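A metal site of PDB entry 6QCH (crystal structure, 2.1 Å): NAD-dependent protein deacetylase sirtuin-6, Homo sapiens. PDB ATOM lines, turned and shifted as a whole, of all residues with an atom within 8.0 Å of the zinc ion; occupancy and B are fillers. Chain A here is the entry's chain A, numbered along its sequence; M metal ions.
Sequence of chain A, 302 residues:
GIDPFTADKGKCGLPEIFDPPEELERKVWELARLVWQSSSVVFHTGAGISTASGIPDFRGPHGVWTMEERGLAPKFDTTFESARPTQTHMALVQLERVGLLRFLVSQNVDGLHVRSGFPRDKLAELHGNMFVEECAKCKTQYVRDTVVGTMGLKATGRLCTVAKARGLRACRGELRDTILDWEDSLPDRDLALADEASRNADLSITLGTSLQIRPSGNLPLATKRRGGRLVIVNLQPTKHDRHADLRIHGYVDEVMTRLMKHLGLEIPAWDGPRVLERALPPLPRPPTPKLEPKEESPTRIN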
ATOM      1  N   GLU A 134     -17.228 -12.990 -25.558  1.00  0.00           N
ATOM      2  CA  GLU A 134     -15.844 -13.273 -26.022  1.00  0.00           C
ATOM      3  C   GLU A 134     -15.079 -11.956 -26.181  1.00  0.00           C
ATOM      4  O   GLU A 134     -15.613 -11.004 -26.759  1.00  0.00           O
ATOM      5  CB  GLU A 134     -15.937 -14.030 -27.352  1.00  0.00           C
ATOM      6  CG  GLU A 134     -14.630 -14.103 -28.099  1.00  0.00           C
ATOM      7  CD  GLU A 134     -14.521 -15.248 -29.091  1.00  0.00           C
ATOM      8  OE1 GLU A 134     -15.355 -16.194 -29.005  1.00  0.00           O
ATOM      9  OE2 GLU A 134     -13.593 -15.208 -29.921  1.00  0.00           O
ATOM     10  N   CYS A 135     -13.844 -11.924 -25.680  1.00  0.00           N
ATOM     11  CA  CYS A 135     -12.940 -10.743 -25.789  1.00  0.00           C
ATOM     12  C   CYS A 135     -12.430 -10.697 -27.237  1.00  0.00           C
ATOM     13  O   CYS A 135     -11.843 -11.688 -27.686  1.00  0.00           O
ATOM     14  CB  CYS A 135     -11.805 -10.810 -24.774  1.00  0.00           C
ATOM     15  SG  CYS A 135     -10.567  -9.492 -24.953  1.00  0.00           S
ATOM     16  N   ALA A 136     -12.597  -9.541 -27.857  1.00  0.00           N
ATOM     17  CA  ALA A 136     -12.094  -9.280 -29.213  1.00  0.00           C
ATOM     18  C   ALA A 136     -10.573  -9.377 -29.181  1.00  0.00           C
ATOM     19  O   ALA A 136      -9.998  -9.841 -30.161  1.00  0.00           O
ATOM     20  CB  ALA A 136     -12.577  -7.928 -29.645  1.00  0.00           C
ATOM     21  N   LYS A 137      -9.963  -8.974 -28.064  1.00  0.00           N
ATOM     22  CA  LYS A 137      -8.479  -8.955 -27.988  1.00  0.00           C
ATOM     23  C   LYS A 137      -7.893 -10.334 -27.680  1.00  0.00           C
ATOM     24  O   LYS A 137      -7.334 -10.900 -28.598  1.00  0.00           O
ATOM     25  CB  LYS A 137      -8.018  -7.941 -26.938  1.00  0.00           C
ATOM     26  N   CYS A 138      -8.093 -10.883 -26.478  1.00  0.00           N
ATOM     27  CA  CYS A 138      -7.502 -12.209 -26.133  1.00  0.00           C
ATOM     28  C   CYS A 138      -8.351 -13.393 -26.626  1.00  0.00           C
ATOM     29  O   CYS A 138      -7.855 -14.521 -26.538  1.00  0.00           O
ATOM     30  CB  CYS A 138      -7.257 -12.354 -24.634  1.00  0.00           C
ATOM     31  SG  CYS A 138      -8.493 -11.586 -23.557  1.00  0.00           S
ATOM     32  N   LYS A 139      -9.593 -13.191 -27.086  1.00  0.00           N
ATOM     33  CA  LYS A 139     -10.514 -14.302 -27.471  1.00  0.00           C
ATOM     34  C   LYS A 139     -10.940 -15.102 -26.228  1.00  0.00           C
ATOM     35  O   LYS A 139     -11.431 -16.252 -26.418  1.00  0.00           O
ATOM     36  CB  LYS A 139      -9.855 -15.279 -28.440  1.00  0.00           C
ATOM     37  CG  LYS A 139      -8.992 -14.640 -29.523  1.00  0.00           C
ATOM     38  CD  LYS A 139      -9.782 -13.756 -30.441  1.00  0.00           C
ATOM     39  CE  LYS A 139     -10.488 -14.560 -31.519  1.00  0.00           C
ATOM     40  NZ  LYS A 139     -10.408 -13.874 -32.832  1.00  0.00           N
ATOM     41  N   THR A 140     -10.782 -14.572 -25.015  1.00  0.00           N
ATOM     42  CA  THR A 140     -11.226 -15.274 -23.775  1.00  0.00           C
ATOM     43  C   THR A 140     -12.763 -15.259 -23.760  1.00  0.00           C
ATOM     44  O   THR A 140     -13.324 -14.167 -24.005  1.00  0.00           O
ATOM     45  CB  THR A 140     -10.672 -14.671 -22.482  1.00  0.00           C
ATOM     46  OG1 THR A 140      -9.312 -15.057 -22.337  1.00  0.00           O
ATOM     47  CG2 THR A 140     -11.441 -15.105 -21.251  1.00  0.00           C
ATOM     48  N   GLN A 141     -13.397 -16.408 -23.532  1.00  0.00           N
ATOM     49  CA  GLN A 141     -14.884 -16.586 -23.485  1.00  0.00           C
ATOM     50  C   GLN A 141     -15.370 -16.556 -22.039  1.00  0.00           C
ATOM     51  O   GLN A 141     -14.643 -17.047 -21.199  1.00  0.00           O
ATOM     52  CB  GLN A 141     -15.269 -17.898 -24.166  1.00  0.00           C
ATOM     53  CG  GLN A 141     -14.864 -17.892 -25.635  1.00  0.00           C
ATOM     54  CD  GLN A 141     -15.708 -18.823 -26.459  1.00  0.00           C
ATOM     55  OE1 GLN A 141     -16.113 -19.882 -25.998  1.00  0.00           O
ATOM     56  NE2 GLN A 141     -15.983 -18.409 -27.691  1.00  0.00           N
ATOM     57  N   TYR A 142     -16.528 -15.957 -21.783  1.00  0.00           N
ATOM     58  CA  TYR A 142     -17.147 -15.812 -20.437  1.00  0.00           C
ATOM     59  C   TYR A 142     -18.528 -16.464 -20.519  1.00  0.00           C
ATOM     60  O   TYR A 142     -19.296 -16.031 -21.360  1.00  0.00           O
ATOM     61  CB  TYR A 142     -17.262 -14.334 -20.045  1.00  0.00           C
ATOM     62  CG  TYR A 142     -15.948 -13.618 -19.832  1.00  0.00           C
ATOM     63  CD1 TYR A 142     -15.164 -13.206 -20.901  1.00  0.00           C
ATOM     64  CD2 TYR A 142     -15.465 -13.374 -18.559  1.00  0.00           C
ATOM     65  CE1 TYR A 142     -13.941 -12.568 -20.714  1.00  0.00           C
ATOM     66  CE2 TYR A 142     -14.257 -12.727 -18.339  1.00  0.00           C
ATOM     67  CZ  TYR A 142     -13.484 -12.317 -19.425  1.00  0.00           C
ATOM     68  OH  TYR A 142     -12.305 -11.666 -19.211  1.00  0.00           O
ATOM     69  N   LEU A 159     -15.948  -5.291 -20.195  1.00  0.00           N
ATOM     70  CA  LEU A 159     -14.499  -5.404 -20.524  1.00  0.00           C
ATOM     71  C   LEU A 159     -13.939  -6.740 -20.011  1.00  0.00           C
ATOM     72  O   LEU A 159     -14.499  -7.310 -19.041  1.00  0.00           O
ATOM     73  CB  LEU A 159     -13.713  -4.228 -19.928  1.00  0.00           C
ATOM     74  CG  LEU A 159     -14.037  -2.832 -20.458  1.00  0.00           C
ATOM     75  CD1 LEU A 159     -12.873  -1.876 -20.196  1.00  0.00           C
ATOM     76  CD2 LEU A 159     -14.390  -2.847 -21.935  1.00  0.00           C
ATOM     77  N   CYS A 160     -12.843  -7.170 -20.626  1.00  0.00           N
ATOM     78  CA  CYS A 160     -12.073  -8.393 -20.281  1.00  0.00           C
ATOM     79  C   CYS A 160     -11.340  -8.225 -18.944  1.00  0.00           C
ATOM     80  O   CYS A 160     -10.788  -7.144 -18.698  1.00  0.00           O
ATOM     81  CB  CYS A 160     -11.083  -8.708 -21.387  1.00  0.00           C
ATOM     82  SG  CYS A 160     -10.419 -10.385 -21.264  1.00  0.00           S
ATOM     83  N   THR A 161     -11.284  -9.271 -18.123  1.00  0.00           N
ATOM     84  CA  THR A 161     -10.788  -9.224 -16.732  1.00  0.00           C
ATOM     85  C   THR A 161      -9.626 -10.213 -16.582  1.00  0.00           C
ATOM     86  O   THR A 161      -9.524 -10.816 -15.522  1.00  0.00           O
ATOM     87  CB  THR A 161     -11.963  -9.465 -15.770  1.00  0.00           C
ATOM     88  OG1 THR A 161     -12.426 -10.811 -15.890  1.00  0.00           O
ATOM     89  CG2 THR A 161     -13.124  -8.530 -16.021  1.00  0.00           C
ATOM     90  N   VAL A 162      -8.799 -10.381 -17.627  1.00  0.00           N
ATOM     91  CA  VAL A 162      -7.706 -11.411 -17.679  1.00  0.00           C
ATOM     92  C   VAL A 162      -6.400 -10.806 -17.143  1.00  0.00           C
ATOM     93  O   VAL A 162      -6.118  -9.642 -17.493  1.00  0.00           O
ATOM     94  CB  VAL A 162      -7.488 -11.964 -19.098  1.00  0.00           C
ATOM     95  CG1 VAL A 162      -6.146 -12.668 -19.230  1.00  0.00           C
ATOM     96  CG2 VAL A 162      -8.611 -12.888 -19.524  1.00  0.00           C
ATOM     97  N   ALA A 163      -5.636 -11.609 -16.389  1.00  0.00           N
ATOM     98  CA  ALA A 163      -4.274 -11.340 -15.863  1.00  0.00           C
ATOM     99  C   ALA A 163      -4.048  -9.831 -15.698  1.00  0.00           C
ATOM    100  O   ALA A 163      -3.065  -9.325 -16.272  1.00  0.00           O
ATOM    101  CB  ALA A 163      -3.229 -11.963 -16.776  1.00  0.00           C
ATOM    102  N   CYS A 171      -6.029  -6.751 -19.111  1.00  0.00           N
ATOM    103  CA  CYS A 171      -6.275  -6.970 -20.566  1.00  0.00           C
ATOM    104  C   CYS A 171      -7.300  -5.949 -21.063  1.00  0.00           C
ATOM    105  O   CYS A 171      -6.976  -5.268 -22.017  1.00  0.00           O
ATOM    106  CB  CYS A 171      -6.765  -8.389 -20.886  1.00  0.00           C
ATOM    107  SG  CYS A 171      -7.321  -8.591 -22.599  1.00  0.00           S
ATOM    108  N   ARG A 172      -8.497  -5.892 -20.446  1.00  0.00           N
ATOM    109  CA  ARG A 172      -9.521  -4.808 -20.604  1.00  0.00           C
ATOM    110  C   ARG A 172     -10.129  -4.775 -22.018  1.00  0.00           C
ATOM    111  O   ARG A 172     -10.888  -3.792 -22.346  1.00  0.00           O
ATOM    112  CB  ARG A 172      -8.938  -3.452 -20.216  1.00  0.00           C
ATOM    113  CG  ARG A 172      -8.494  -3.350 -18.763  1.00  0.00           C
ATOM    114  CD  ARG A 172      -8.415  -1.916 -18.274  1.00  0.00           C
ATOM    115  NE  ARG A 172      -9.733  -1.274 -18.281  1.00  0.00           N
ATOM    116  CZ  ARG A 172      -9.947   0.039 -18.305  1.00  0.00           C
ATOM    117  NH1 ARG A 172      -8.931   0.897 -18.340  1.00  0.00           N
ATOM    118  NH2 ARG A 172     -11.188   0.502 -18.311  1.00  0.00           N
ATOM    119  N   GLY A 173      -9.880  -5.818 -22.817  1.00  0.00           N
ATOM    120  CA  GLY A 173     -10.482  -5.983 -24.157  1.00  0.00           C
ATOM    121  C   GLY A 173     -11.994  -5.809 -24.086  1.00  0.00           C
ATOM    122  O   GLY A 173     -12.579  -6.136 -23.028  1.00  0.00           O
ATOM    123  N   GLU A 174     -12.590  -5.315 -25.181  1.00  0.00           N
ATOM    124  CA  GLU A 174     -14.053  -5.142 -25.383  1.00  0.00           C
ATOM    125  C   GLU A 174     -14.685  -6.538 -25.528  1.00  0.00           C
ATOM    126  O   GLU A 174     -14.116  -7.381 -26.278  1.00  0.00           O
ATOM    127  CB  GLU A 174     -14.329  -4.261 -26.601  1.00  0.00           C
ATOM    128  CG  GLU A 174     -15.791  -3.874 -26.788  1.00  0.00           C
ATOM    129  CD  GLU A 174     -16.023  -2.964 -27.991  1.00  0.00           C
ATOM    130  OE1 GLU A 174     -15.588  -1.799 -27.935  1.00  0.00           O
ATOM    131  OE2 GLU A 174     -16.622  -3.432 -28.998  1.00  0.00           O
ATOM    132  N   LEU A 175     -15.779  -6.774 -24.789  1.00  0.00           N
ATOM    133  CA  LEU A 175     -16.532  -8.053 -24.765  1.00  0.00           C
ATOM    134  C   LEU A 175     -17.703  -7.940 -25.751  1.00  0.00           C
ATOM    135  O   LEU A 175     -18.352  -6.888 -25.812  1.00  0.00           O
ATOM    136  CB  LEU A 175     -17.038  -8.394 -23.359  1.00  0.00           C
ATOM    137  CG  LEU A 175     -15.957  -8.684 -22.311  1.00  0.00           C
ATOM    138  CD1 LEU A 175     -16.575  -9.211 -21.020  1.00  0.00           C
ATOM    139  CD2 LEU A 175     -14.911  -9.648 -22.848  1.00  0.00           C
HETATM  140 ZN    ZN M   1      -9.378  -9.988 -23.125  1.00  0.00          ZN
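The backbone NH (N) of Arg 172 sits at hydrogen-bond distance from the backbone carbonyl oxygen (O) of Cys 160.
The backbone carbonyl oxygen of Gly 173 lies within hydrogen-bond range of the backbone NH of Cys 160.
OH of Tyr 142 sits close to SG of Cys 160, at 3.1 Å.
The side-chain sulfur (SG) of Cys 171 sits close to the backbone NH (N) of Gly 173 (3.8 Å).
O of Thr 140 is in hydrogen-bond range of N of Cys 135 (2.8 Å).
N of Cys 171 is in hydrogen-bond range of O of Val 162 (3.3 Å).
The side-chain sulfur (SG) of Cys 135 sits close to the backbone NH (N) of Lys 137 (3.2 Å).
The side-chain hydroxyl of Thr 140 lies close to the side-chain sulfur of Cys 138, at 3.8 Å.
The zinc ion is bound by SG of Cys 138 (1.9 Å), SG of Cys 160 (2.2 Å), SG of Cys 135 (2.2 Å) and SG of Cys 171 (2.5 Å).
Within 4 Å of the zinc ion: Cys 135, Cys 138, Cys 160 and Cys 171.
The nearest printed residue that does not touch the zinc ion is Gly 173 (4.2 Å).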
